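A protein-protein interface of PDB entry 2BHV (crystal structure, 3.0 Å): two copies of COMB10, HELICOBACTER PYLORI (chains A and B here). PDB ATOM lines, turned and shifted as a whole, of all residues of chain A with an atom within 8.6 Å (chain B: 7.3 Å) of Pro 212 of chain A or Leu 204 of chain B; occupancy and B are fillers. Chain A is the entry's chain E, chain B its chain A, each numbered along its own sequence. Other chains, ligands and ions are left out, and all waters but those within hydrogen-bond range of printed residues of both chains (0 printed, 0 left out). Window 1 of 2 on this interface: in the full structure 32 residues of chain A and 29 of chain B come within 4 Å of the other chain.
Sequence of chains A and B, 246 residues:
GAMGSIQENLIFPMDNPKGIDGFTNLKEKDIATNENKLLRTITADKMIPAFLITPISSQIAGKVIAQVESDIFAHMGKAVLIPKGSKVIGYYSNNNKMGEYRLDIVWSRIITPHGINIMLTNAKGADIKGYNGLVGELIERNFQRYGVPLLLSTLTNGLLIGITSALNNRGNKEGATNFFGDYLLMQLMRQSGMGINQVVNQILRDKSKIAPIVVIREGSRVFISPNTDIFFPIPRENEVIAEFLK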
ATOM      1  N   SER A  57     -19.314 -21.541  31.814  1.00  0.00           N
ATOM      2  CA  SER A  57     -17.948 -21.432  31.249  1.00  0.00           C
ATOM      3  C   SER A  57     -17.908 -20.504  30.024  1.00  0.00           C
ATOM      4  O   SER A  57     -18.890 -20.410  29.288  1.00  0.00           O
ATOM      5  CB  SER A  57     -17.391 -22.816  30.884  1.00  0.00           C
ATOM      6  OG  SER A  57     -18.182 -23.452  29.892  1.00  0.00           O
ATOM      7  N   SER A  58     -16.776 -19.830  29.798  1.00  0.00           N
ATOM      8  CA  SER A  58     -16.677 -18.844  28.697  1.00  0.00           C
ATOM      9  C   SER A  58     -16.316 -19.414  27.316  1.00  0.00           C
ATOM     10  O   SER A  58     -16.456 -18.716  26.304  1.00  0.00           O
ATOM     11  CB  SER A  58     -15.740 -17.681  29.053  1.00  0.00           C
ATOM     12  OG  SER A  58     -14.380 -18.051  28.888  1.00  0.00           O
ATOM     13  N   GLN A  59     -15.830 -20.654  27.267  1.00  0.00           N
ATOM     14  CA  GLN A  59     -15.654 -21.323  25.975  1.00  0.00           C
ATOM     15  C   GLN A  59     -17.010 -21.887  25.552  1.00  0.00           C
ATOM     16  O   GLN A  59     -17.706 -21.287  24.729  1.00  0.00           O
ATOM     17  CB  GLN A  59     -14.583 -22.431  26.012  1.00  0.00           C
ATOM     18  CG  GLN A  59     -13.394 -22.212  26.964  1.00  0.00           C
ATOM     19  CD  GLN A  59     -13.306 -23.291  28.050  1.00  0.00           C
ATOM     20  OE1 GLN A  59     -14.065 -23.275  29.033  1.00  0.00           O
ATOM     21  NE2 GLN A  59     -12.378 -24.237  27.872  1.00  0.00           N
ATOM     22  N   ASN A  94     -21.208 -17.137  24.984  1.00  0.00           N
ATOM     23  CA  ASN A  94     -20.212 -16.095  25.031  1.00  0.00           C
ATOM     24  C   ASN A  94     -19.940 -15.586  23.620  1.00  0.00           C
ATOM     25  O   ASN A  94     -19.718 -16.373  22.699  1.00  0.00           O
ATOM     26  CB  ASN A  94     -18.949 -16.584  25.742  1.00  0.00           C
ATOM     27  CG  ASN A  94     -19.139 -16.688  27.254  1.00  0.00           C
ATOM     28  OD1 ASN A  94     -19.392 -17.771  27.791  1.00  0.00           O
ATOM     29  ND2 ASN A  94     -19.043 -15.549  27.941  1.00  0.00           N
ATOM     30  N   ASN A  95     -20.103 -14.276  23.435  1.00  0.00           N
ATOM     31  CA  ASN A  95     -19.514 -13.563  22.307  1.00  0.00           C
ATOM     32  C   ASN A  95     -18.180 -13.025  22.791  1.00  0.00           C
ATOM     33  O   ASN A  95     -17.805 -13.236  23.951  1.00  0.00           O
ATOM     34  CB  ASN A  95     -20.378 -12.367  21.899  1.00  0.00           C
ATOM     35  CG  ASN A  95     -21.666 -12.774  21.225  1.00  0.00           C
ATOM     36  OD1 ASN A  95     -22.611 -13.238  21.906  1.00  0.00           O
ATOM     37  ND2 ASN A  95     -21.727 -12.573  19.876  1.00  0.00           N
ATOM     38  N   ASN A  96     -17.465 -12.340  21.906  1.00  0.00           N
ATOM     39  CA  ASN A  96     -16.438 -11.371  22.317  1.00  0.00           C
ATOM     40  C   ASN A  96     -15.545 -10.859  21.180  1.00  0.00           C
ATOM     41  O   ASN A  96     -15.238 -11.597  20.233  1.00  0.00           O
ATOM     42  CB  ASN A  96     -15.616 -11.818  23.563  1.00  0.00           C
ATOM     43  CG  ASN A  96     -14.788 -13.085  23.334  1.00  0.00           C
ATOM     44  OD1 ASN A  96     -15.322 -14.202  23.313  1.00  0.00           O
ATOM     45  ND2 ASN A  96     -13.471 -12.915  23.207  1.00  0.00           N
ATOM     46  N   MET A  98     -12.350 -10.196  21.186  1.00  0.00           N
ATOM     47  CA  MET A  98     -10.945 -10.521  21.525  1.00  0.00           C
ATOM     48  C   MET A  98     -10.450  -9.888  22.835  1.00  0.00           C
ATOM     49  O   MET A  98      -9.713  -8.902  22.834  1.00  0.00           O
ATOM     50  CB  MET A  98     -10.004 -10.216  20.343  1.00  0.00           C
ATOM     51  CG  MET A  98     -10.475 -10.836  19.038  1.00  0.00           C
ATOM     52  SD  MET A  98      -9.341 -10.548  17.649  1.00  0.00           S
ATOM     53  CE  MET A  98     -10.744 -10.451  16.245  1.00  0.00           C
ATOM     54  N   GLY A  99     -10.868 -10.481  23.952  1.00  0.00           N
ATOM     55  CA  GLY A  99     -10.575  -9.955  25.292  1.00  0.00           C
ATOM     56  C   GLY A  99     -11.799  -9.321  25.948  1.00  0.00           C
ATOM     57  O   GLY A  99     -11.996  -9.450  27.175  1.00  0.00           O
ATOM     58  N   GLU A 100     -12.618  -8.652  25.116  1.00  0.00           N
ATOM     59  CA  GLU A 100     -13.798  -7.860  25.553  1.00  0.00           C
ATOM     60  C   GLU A 100     -15.076  -8.711  25.779  1.00  0.00           C
ATOM     61  O   GLU A 100     -15.893  -8.898  24.863  1.00  0.00           O
ATOM     62  CB  GLU A 100     -14.060  -6.710  24.556  1.00  0.00           C
ATOM     63  CG  GLU A 100     -14.599  -5.410  25.175  1.00  0.00           C
ATOM     64  CD  GLU A 100     -16.060  -5.496  25.596  1.00  0.00           C
ATOM     65  OE1 GLU A 100     -16.865  -6.113  24.862  1.00  0.00           O
ATOM     66  OE2 GLU A 100     -16.406  -4.938  26.660  1.00  0.00           O
ATOM     67  N   TYR A 101     -15.235  -9.178  27.021  1.00  0.00           N
ATOM     68  CA  TYR A 101     -16.209 -10.204  27.436  1.00  0.00           C
ATOM     69  C   TYR A 101     -17.679  -9.884  27.141  1.00  0.00           C
ATOM     70  O   TYR A 101     -18.185  -8.827  27.530  1.00  0.00           O
ATOM     71  CB  TYR A 101     -16.020 -10.451  28.938  1.00  0.00           C
ATOM     72  CG  TYR A 101     -16.888 -11.516  29.557  1.00  0.00           C
ATOM     73  CD1 TYR A 101     -18.123 -11.195  30.129  1.00  0.00           C
ATOM     74  CD2 TYR A 101     -16.460 -12.841  29.614  1.00  0.00           C
ATOM     75  CE1 TYR A 101     -18.915 -12.172  30.722  1.00  0.00           C
ATOM     76  CE2 TYR A 101     -17.249 -13.828  30.199  1.00  0.00           C
ATOM     77  CZ  TYR A 101     -18.473 -13.490  30.753  1.00  0.00           C
ATOM     78  OH  TYR A 101     -19.249 -14.464  31.343  1.00  0.00           O
ATOM     79  N   ARG A 102     -18.358 -10.808  26.457  1.00  0.00           N
ATOM     80  CA  ARG A 102     -19.811 -10.717  26.282  1.00  0.00           C
ATOM     81  C   ARG A 102     -20.558 -12.032  26.568  1.00  0.00           C
ATOM     82  O   ARG A 102     -20.356 -13.047  25.888  1.00  0.00           O
ATOM     83  CB  ARG A 102     -20.177 -10.184  24.894  1.00  0.00           C
ATOM     84  CG  ARG A 102     -21.666 -10.323  24.564  1.00  0.00           C
ATOM     85  CD  ARG A 102     -22.541  -9.336  25.353  1.00  0.00           C
ATOM     86  NE  ARG A 102     -22.616  -8.050  24.673  1.00  0.00           N
ATOM     87  CZ  ARG A 102     -23.392  -7.810  23.619  1.00  0.00           C
ATOM     88  NH1 ARG A 102     -24.174  -8.769  23.132  1.00  0.00           N
ATOM     89  NH2 ARG A 102     -23.388  -6.610  23.049  1.00  0.00           N
ATOM     90  N   ILE A 161     -16.242 -15.745  40.380  1.00  0.00           N
ATOM     91  CA  ILE A 161     -15.616 -15.673  39.059  1.00  0.00           C
ATOM     92  C   ILE A 161     -14.175 -16.162  39.020  1.00  0.00           C
ATOM     93  O   ILE A 161     -13.294 -15.556  39.632  1.00  0.00           O
ATOM     94  CB  ILE A 161     -15.629 -14.239  38.508  1.00  0.00           C
ATOM     95  CG1 ILE A 161     -17.058 -13.681  38.474  1.00  0.00           C
ATOM     96  CG2 ILE A 161     -14.994 -14.201  37.116  1.00  0.00           C
ATOM     97  CD1 ILE A 161     -17.127 -12.162  38.522  1.00  0.00           C
ATOM     98  N   GLY A 162     -13.944 -17.238  38.267  1.00  0.00           N
ATOM     99  CA  GLY A 162     -12.595 -17.769  38.010  1.00  0.00           C
ATOM    100  C   GLY A 162     -12.131 -17.362  36.626  1.00  0.00           C
ATOM    101  O   GLY A 162     -12.884 -17.451  35.667  1.00  0.00           O
ATOM    102  N   ILE A 163     -10.877 -16.953  36.501  1.00  0.00           N
ATOM    103  CA  ILE A 163     -10.501 -16.067  35.389  1.00  0.00           C
ATOM    104  C   ILE A 163      -9.160 -16.370  34.667  1.00  0.00           C
ATOM    105  O   ILE A 163      -8.341 -15.473  34.479  1.00  0.00           O
ATOM    106  CB  ILE A 163     -10.577 -14.574  35.895  1.00  0.00           C
ATOM    107  CG1 ILE A 163     -10.846 -13.601  34.754  1.00  0.00           C
ATOM    108  CG2 ILE A 163      -9.355 -14.186  36.792  1.00  0.00           C
ATOM    109  CD1 ILE A 163     -11.610 -12.386  35.210  1.00  0.00           C
ATOM    110  N   THR A 164      -8.956 -17.618  34.233  1.00  0.00           N
ATOM    111  CA  THR A 164      -7.648 -18.048  33.679  1.00  0.00           C
ATOM    112  C   THR A 164      -7.371 -17.581  32.237  1.00  0.00           C
ATOM    113  O   THR A 164      -8.302 -17.350  31.455  1.00  0.00           O
ATOM    114  CB  THR A 164      -7.477 -19.583  33.749  1.00  0.00           C
ATOM    115  OG1 THR A 164      -8.026 -20.065  34.976  1.00  0.00           O
ATOM    116  CG2 THR A 164      -6.000 -19.967  33.686  1.00  0.00           C
ATOM    117  N   SER A 165      -6.085 -17.443  31.901  1.00  0.00           N
ATOM    118  CA  SER A 165      -5.662 -17.185  30.517  1.00  0.00           C
ATOM    119  C   SER A 165      -5.315 -18.498  29.793  1.00  0.00           C
ATOM    120  O   SER A 165      -4.726 -19.403  30.393  1.00  0.00           O
ATOM    121  CB  SER A 165      -4.482 -16.199  30.474  1.00  0.00           C
ATOM    122  N   ALA A 166      -5.689 -18.583  28.511  1.00  0.00           N
ATOM    123  CA  ALA A 166      -5.554 -19.810  27.696  1.00  0.00           C
ATOM    124  C   ALA A 166      -4.114 -20.304  27.481  1.00  0.00           C
ATOM    125  O   ALA A 166      -3.870 -21.516  27.470  1.00  0.00           O
ATOM    126  CB  ALA A 166      -6.265 -19.637  26.350  1.00  0.00           C
ATOM    127  N   LEU A 167      -3.175 -19.367  27.301  1.00  0.00           N
ATOM    128  CA  LEU A 167      -1.742 -19.694  27.159  1.00  0.00           C
ATOM    129  C   LEU A 167      -0.956 -19.312  28.410  1.00  0.00           C
ATOM    130  O   LEU A 167       0.157 -19.789  28.619  1.00  0.00           O
ATOM    131  CB  LEU A 167      -1.140 -19.013  25.921  1.00  0.00           C
ATOM    132  N   LYS A 207      -0.654 -10.181  23.009  1.00  0.00           N
ATOM    133  CA  LYS A 207      -1.016 -11.148  24.057  1.00  0.00           C
ATOM    134  C   LYS A 207      -2.435 -10.998  24.572  1.00  0.00           C
ATOM    135  O   LYS A 207      -2.838 -11.701  25.496  1.00  0.00           O
ATOM    136  CB  LYS A 207      -0.043 -11.084  25.230  1.00  0.00           C
ATOM    137  CG  LYS A 207       0.915 -12.242  25.259  1.00  0.00           C
ATOM    138  CD  LYS A 207       1.448 -12.476  26.658  1.00  0.00           C
ATOM    139  CE  LYS A 207       2.595 -13.469  26.636  1.00  0.00           C
ATOM    140  NZ  LYS A 207       3.690 -13.014  25.727  1.00  0.00           N
ATOM    141  N   SER A 208      -3.193 -10.096  23.964  1.00  0.00           N
ATOM    142  CA  SER A 208      -4.537  -9.807  24.432  1.00  0.00           C
ATOM    143  C   SER A 208      -5.580  -9.849  23.314  1.00  0.00           C
ATOM    144  O   SER A 208      -6.576  -9.122  23.356  1.00  0.00           O
ATOM    145  CB  SER A 208      -4.552  -8.459  25.152  1.00  0.00           C
ATOM    146  OG  SER A 208      -3.549  -8.431  26.157  1.00  0.00           O
ATOM    147  N   LYS A 209      -5.340 -10.690  22.310  1.00  0.00           N
ATOM    148  CA  LYS A 209      -6.366 -11.027  21.327  1.00  0.00           C
ATOM    149  C   LYS A 209      -7.002 -12.294  21.843  1.00  0.00           C
ATOM    150  O   LYS A 209      -8.230 -12.448  21.847  1.00  0.00           O
ATOM    151  CB  LYS A 209      -5.755 -11.289  19.946  1.00  0.00           C
ATOM    152  CG  LYS A 209      -4.865 -10.177  19.394  1.00  0.00           C
ATOM    153  CD  LYS A 209      -5.659  -8.920  19.064  1.00  0.00           C
ATOM    154  CE  LYS A 209      -4.730  -7.785  18.677  1.00  0.00           C
ATOM    155  NZ  LYS A 209      -5.468  -6.499  18.563  1.00  0.00           N
ATOM    156  N   ILE A 210      -6.138 -13.196  22.294  1.00  0.00           N
ATOM    157  CA  ILE A 210      -6.548 -14.437  22.908  1.00  0.00           C
ATOM    158  C   ILE A 210      -7.440 -14.103  24.106  1.00  0.00           C
ATOM    159  O   ILE A 210      -6.980 -13.521  25.093  1.00  0.00           O
ATOM    160  CB  ILE A 210      -5.314 -15.293  23.332  1.00  0.00           C
ATOM    161  CG1 ILE A 210      -4.472 -15.709  22.106  1.00  0.00           C
ATOM    162  CG2 ILE A 210      -5.756 -16.539  24.100  1.00  0.00           C
ATOM    163  CD1 ILE A 210      -3.377 -14.718  21.679  1.00  0.00           C
ATOM    164  N   ALA A 211      -8.727 -14.437  23.988  1.00  0.00           N
ATOM    165  CA  ALA A 211      -9.688 -14.207  25.068  1.00  0.00           C
ATOM    166  C   ALA A 211      -9.393 -15.112  26.263  1.00  0.00           C
ATOM    167  O   ALA A 211      -9.114 -16.304  26.097  1.00  0.00           O
ATOM    168  CB  ALA A 211     -11.119 -14.413  24.574  1.00  0.00           C
ATOM    169  N   PRO A 212      -9.419 -14.534  27.468  1.00  0.00           N
ATOM    170  CA  PRO A 212      -9.284 -15.303  28.719  1.00  0.00           C
ATOM    171  C   PRO A 212     -10.453 -16.284  28.955  1.00  0.00           C
ATOM    172  O   PRO A 212     -11.587 -15.997  28.558  1.00  0.00           O
ATOM    173  CB  PRO A 212      -9.269 -14.214  29.807  1.00  0.00           C
ATOM    174  CG  PRO A 212      -9.886 -13.007  29.164  1.00  0.00           C
ATOM    175  CD  PRO A 212      -9.549 -13.084  27.707  1.00  0.00           C
ATOM    176  N   ILE A 213     -10.173 -17.426  29.587  1.00  0.00           N
ATOM    177  CA  ILE A 213     -11.241 -18.341  30.003  1.00  0.00           C
ATOM    178  C   ILE A 213     -11.866 -17.861  31.324  1.00  0.00           C
ATOM    179  O   ILE A 213     -11.235 -17.896  32.384  1.00  0.00           O
ATOM    180  CB  ILE A 213     -10.774 -19.841  30.058  1.00  0.00           C
ATOM    181  CG1 ILE A 213     -10.490 -20.367  28.652  1.00  0.00           C
ATOM    182  CG2 ILE A 213     -11.827 -20.745  30.721  1.00  0.00           C
ATOM    183  CD1 ILE A 213      -9.092 -20.126  28.203  1.00  0.00           C
ATOM    184  N   VAL A 214     -13.106 -17.389  31.226  1.00  0.00           N
ATOM    185  CA  VAL A 214     -13.884 -16.920  32.374  1.00  0.00           C
ATOM    186  C   VAL A 214     -14.964 -17.928  32.768  1.00  0.00           C
ATOM    187  O   VAL A 214     -15.806 -18.312  31.953  1.00  0.00           O
ATOM    188  CB  VAL A 214     -14.582 -15.573  32.083  1.00  0.00           C
ATOM    189  CG1 VAL A 214     -15.404 -15.125  33.296  1.00  0.00           C
ATOM    190  CG2 VAL A 214     -13.570 -14.519  31.693  1.00  0.00           C
ATOM    191  N   VAL A 215     -14.937 -18.349  34.024  1.00  0.00           N
ATOM    192  CA  VAL A 215     -15.967 -19.224  34.533  1.00  0.00           C
ATOM    193  C   VAL A 215     -16.706 -18.513  35.652  1.00  0.00           C
ATOM    194  O   VAL A 215     -16.090 -17.876  36.508  1.00  0.00           O
ATOM    195  CB  VAL A 215     -15.394 -20.574  35.004  1.00  0.00           C
ATOM    196  CG1 VAL A 215     -16.413 -21.339  35.844  1.00  0.00           C
ATOM    197  CG2 VAL A 215     -14.969 -21.406  33.806  1.00  0.00           C
ATOM    198  N   VAL B 199     -19.507  -6.337  35.132  1.00  0.00           N
ATOM    199  CA  VAL B 199     -18.548  -6.667  36.188  1.00  0.00           C
ATOM    200  C   VAL B 199     -17.334  -7.435  35.657  1.00  0.00           C
ATOM    201  O   VAL B 199     -16.211  -7.201  36.100  1.00  0.00           O
ATOM    202  CB  VAL B 199     -19.193  -7.446  37.361  1.00  0.00           C
ATOM    203  CG1 VAL B 199     -20.277  -6.619  38.043  1.00  0.00           C
ATOM    204  CG2 VAL B 199     -19.747  -8.777  36.894  1.00  0.00           C
ATOM    205  N   VAL B 200     -17.560  -8.349  34.711  1.00  0.00           N
ATOM    206  CA  VAL B 200     -16.470  -9.158  34.161  1.00  0.00           C
ATOM    207  C   VAL B 200     -15.554  -8.305  33.297  1.00  0.00           C
ATOM    208  O   VAL B 200     -14.337  -8.447  33.366  1.00  0.00           O
ATOM    209  CB  VAL B 200     -16.969 -10.382  33.351  1.00  0.00           C
ATOM    210  CG1 VAL B 200     -15.784 -11.232  32.885  1.00  0.00           C
ATOM    211  CG2 VAL B 200     -17.909 -11.231  34.179  1.00  0.00           C
ATOM    212  N   ASN B 201     -16.136  -7.419  32.491  1.00  0.00           N
ATOM    213  CA  ASN B 201     -15.343  -6.499  31.668  1.00  0.00           C
ATOM    214  C   ASN B 201     -14.489  -5.569  32.526  1.00  0.00           C
ATOM    215  O   ASN B 201     -13.303  -5.362  32.236  1.00  0.00           O
ATOM    216  CB  ASN B 201     -16.234  -5.697  30.708  1.00  0.00           C
ATOM    217  CG  ASN B 201     -16.682  -6.515  29.497  1.00  0.00           C
ATOM    218  OD1 ASN B 201     -15.872  -7.166  28.839  1.00  0.00           O
ATOM    219  ND2 ASN B 201     -17.978  -6.469  29.197  1.00  0.00           N
ATOM    220  N   GLN B 202     -15.096  -5.042  33.596  1.00  0.00           N
ATOM    221  CA  GLN B 202     -14.398  -4.186  34.564  1.00  0.00           C
ATOM    222  C   GLN B 202     -13.225  -4.887  35.270  1.00  0.00           C
ATOM    223  O   GLN B 202     -12.103  -4.356  35.288  1.00  0.00           O
ATOM    224  CB  GLN B 202     -15.369  -3.562  35.582  1.00  0.00           C
ATOM    225  CG  GLN B 202     -14.725  -2.579  36.593  1.00  0.00           C
ATOM    226  CD  GLN B 202     -13.709  -1.616  35.957  1.00  0.00           C
ATOM    227  OE1 GLN B 202     -14.024  -0.865  35.019  1.00  0.00           O
ATOM    228  NE2 GLN B 202     -12.481  -1.633  36.474  1.00  0.00           N
ATOM    229  N   ILE B 203     -13.479  -6.068  35.839  1.00  0.00           N
ATOM    230  CA  ILE B 203     -12.399  -6.891  36.390  1.00  0.00           C
ATOM    231  C   ILE B 203     -11.278  -7.102  35.347  1.00  0.00           C
ATOM    232  O   ILE B 203     -10.100  -6.883  35.644  1.00  0.00           O
ATOM    233  CB  ILE B 203     -12.917  -8.259  36.926  1.00  0.00           C
ATOM    234  CG1 ILE B 203     -13.829  -8.060  38.148  1.00  0.00           C
ATOM    235  CG2 ILE B 203     -11.753  -9.169  37.280  1.00  0.00           C
ATOM    236  CD1 ILE B 203     -14.335  -9.352  38.778  1.00  0.00           C
ATOM    237  N   LEU B 204     -11.650  -7.497  34.129  1.00  0.00           N
ATOM    238  CA  LEU B 204     -10.669  -7.770  33.071  1.00  0.00           C
ATOM    239  C   LEU B 204      -9.851  -6.541  32.659  1.00  0.00           C
ATOM    240  O   LEU B 204      -8.619  -6.624  32.537  1.00  0.00           O
ATOM    241  CB  LEU B 204     -11.338  -8.402  31.843  1.00  0.00           C
ATOM    242  CG  LEU B 204     -11.584  -9.915  31.846  1.00  0.00           C
ATOM    243  CD1 LEU B 204     -12.431 -10.298  30.640  1.00  0.00           C
ATOM    244  CD2 LEU B 204     -10.279 -10.716  31.860  1.00  0.00           C
ATOM    245  N   ARG B 205     -10.537  -5.410  32.441  1.00  0.00           N
ATOM    246  CA  ARG B 205      -9.860  -4.146  32.138  1.00  0.00           C
ATOM    247  C   ARG B 205      -8.871  -3.780  33.241  1.00  0.00           C
ATOM    248  O   ARG B 205      -7.688  -3.545  32.962  1.00  0.00           O
ATOM    249  CB  ARG B 205     -10.857  -3.020  31.904  1.00  0.00           C
ATOM    250  CG  ARG B 205     -11.080  -2.712  30.437  1.00  0.00           C
ATOM    251  CD  ARG B 205     -11.851  -1.419  30.279  1.00  0.00           C
ATOM    252  NE  ARG B 205     -13.087  -1.466  31.055  1.00  0.00           N
ATOM    253  CZ  ARG B 205     -14.298  -1.668  30.549  1.00  0.00           C
ATOM    254  NH1 ARG B 205     -14.478  -1.819  29.243  1.00  0.00           N
ATOM    255  NH2 ARG B 205     -15.334  -1.711  31.365  1.00  0.00           N
ATOM    256  N   ASP B 206      -9.350  -3.771  34.491  1.00  0.00           N
ATOM    257  CA  ASP B 206      -8.472  -3.622  35.654  1.00  0.00           C
ATOM    258  C   ASP B 206      -7.257  -4.531  35.596  1.00  0.00           C
ATOM    259  O   ASP B 206      -6.206  -4.171  36.105  1.00  0.00           O
ATOM    260  CB  ASP B 206      -9.224  -3.861  36.963  1.00  0.00           C
ATOM    261  CG  ASP B 206      -9.241  -2.635  37.861  1.00  0.00           C
ATOM    262  OD1 ASP B 206      -9.111  -1.505  37.329  1.00  0.00           O
ATOM    263  OD2 ASP B 206      -9.394  -2.803  39.104  1.00  0.00           O
ATOM    264  N   LYS B 207      -7.399  -5.706  34.978  1.00  0.00           N
ATOM    265  CA  LYS B 207      -6.286  -6.658  34.879  1.00  0.00           C
ATOM    266  C   LYS B 207      -5.112  -6.147  34.030  1.00  0.00           C
ATOM    267  O   LYS B 207      -3.957  -6.275  34.435  1.00  0.00           O
ATOM    268  CB  LYS B 207      -6.756  -8.030  34.388  1.00  0.00           C
ATOM    269  CG  LYS B 207      -7.118  -9.000  35.496  1.00  0.00           C
ATOM    270  CD  LYS B 207      -6.833 -10.432  35.046  1.00  0.00           C
ATOM    271  CE  LYS B 207      -6.892 -11.433  36.215  1.00  0.00           C
ATOM    272  NZ  LYS B 207      -6.151 -12.709  35.916  1.00  0.00           N
ATOM    273  N   SER B 208      -5.390  -5.555  32.873  1.00  0.00           N
ATOM    274  CA  SER B 208      -4.293  -4.981  32.084  1.00  0.00           C
ATOM    275  C   SER B 208      -3.753  -3.662  32.680  1.00  0.00           C
ATOM    276  O   SER B 208      -2.745  -3.132  32.209  1.00  0.00           O
ATOM    277  CB  SER B 208      -4.663  -4.827  30.596  1.00  0.00           C
ATOM    278  OG  SER B 208      -5.423  -3.658  30.362  1.00  0.00           O
ATOM    279  N   LYS B 209      -4.419  -3.153  33.719  1.00  0.00           N
ATOM    280  CA  LYS B 209      -4.002  -1.900  34.373  1.00  0.00           C
ATOM    281  C   LYS B 209      -2.562  -1.976  34.897  1.00  0.00           C
ATOM    282  O   LYS B 209      -1.741  -1.110  34.584  1.00  0.00           O
ATOM    283  CB  LYS B 209      -4.980  -1.465  35.494  1.00  0.00           C
ATOM    284  CG  LYS B 209      -6.072  -0.443  35.069  1.00  0.00           C
ATOM    285  CD  LYS B 209      -6.277   0.624  36.160  1.00  0.00           C
ATOM    286  CE  LYS B 209      -7.729   1.097  36.274  1.00  0.00           C
ATOM    287  NZ  LYS B 209      -8.192   1.908  35.114  1.00  0.00           N
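The side-chain carboxylate of Glu 100 of chain A lies close to the side-chain amide oxygen of Asn 201 of chain B, 3.2 Å away.
The backbone NH (N) of Tyr 101 of chain A lies within hydrogen-bond range of the side-chain amide oxygen (OD1) of Asn 201 of chain B (2.8 Å).
The side-chain hydroxyl of Ser 58 of chain A lies within hydrogen-bond range of the backbone carbonyl oxygen of Pro 212 of chain A, 3.5 Å away.
The side-chain hydroxyl (OG) of Ser 58 of chain A lies within hydrogen-bond range of the backbone NH (N) of Val 214 of chain A, at 2.7 Å.
Gly 99 of chain A touches Leu 204 of chain B (O to CD1, 3.6 Å).
Val 200 of chain B touches Tyr 101 of chain A.
CD1 of Leu 204 of chain B touches CB of Tyr 101 of chain A (3.98 Å).
CD1 of Ile 203 of chain B touches CD1 of Ile 161 of chain A (3.97 Å).
Ile 203 of chain B touches Ile 163 of chain A.
Leu 204 of chain B touches Ile 163 of chain A (CD2 to CD1, 3.97 Å).
NZ of Lys 207 of chain B touches CG2 of Ile 163 of chain A (3.6 Å).
Leu 204 of chain B touches Pro 212 of chain A (CD2 to CG, 3.6 Å).
Val 214 of chain A touches Val 200 of chain B (CG1 to CG1, 3.9 Å).
Of chain B, only Leu 204 (3.6 Å) comes within 4 Å of Pro 212 of chain A.
Leu 204 of chain B touches just these residues of chain A: Gly 99 (3.6 Å), Tyr 101 (3.98 Å), Ile 163 (3.97 Å) and Pro 212 (3.6 Å).
Of the printed residues of chain B, Ile 161 of chain A touches Ile 203 (3.97 Å).
Printed residues of chain B within 4 Å of Gly 99 of chain A: Leu 204 (3.6 Å).
Thr 164 of chain A touches none of the printed residues of chain B.
The nearest residue of chain A that does not touch Leu 204 of chain B is Val 214 of chain A (4.5 Å).
The nearest printed residue of chain B that does not touch Ile 163 of chain A is Val 200 of chain B (4.9 Å).
Printed residues of chain B that touch a printed residue of chain A: Val 200, Asn 201, Ile 203, Leu 204 and Lys 207.
Of the 27 printed residues of chain A, 7 touch a printed residue of chain B.
Hydrophobic or aromatic side chains of chain A within 4 Å of the printed part of chain B: Tyr 101, Ile 161, Ile 163, Pro 212 and Val 214.
Along chain A the printed residues that touch a printed residue of chain B span positions 99 to 214.
Among the printed residues, 11 pairs touch across the chains.
Among the printed residues, no Asp or Glu carboxylate lies within 4 Å of a Lys or Arg side-chain nitrogen of the other chain.
3 positions are printed for both chains.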
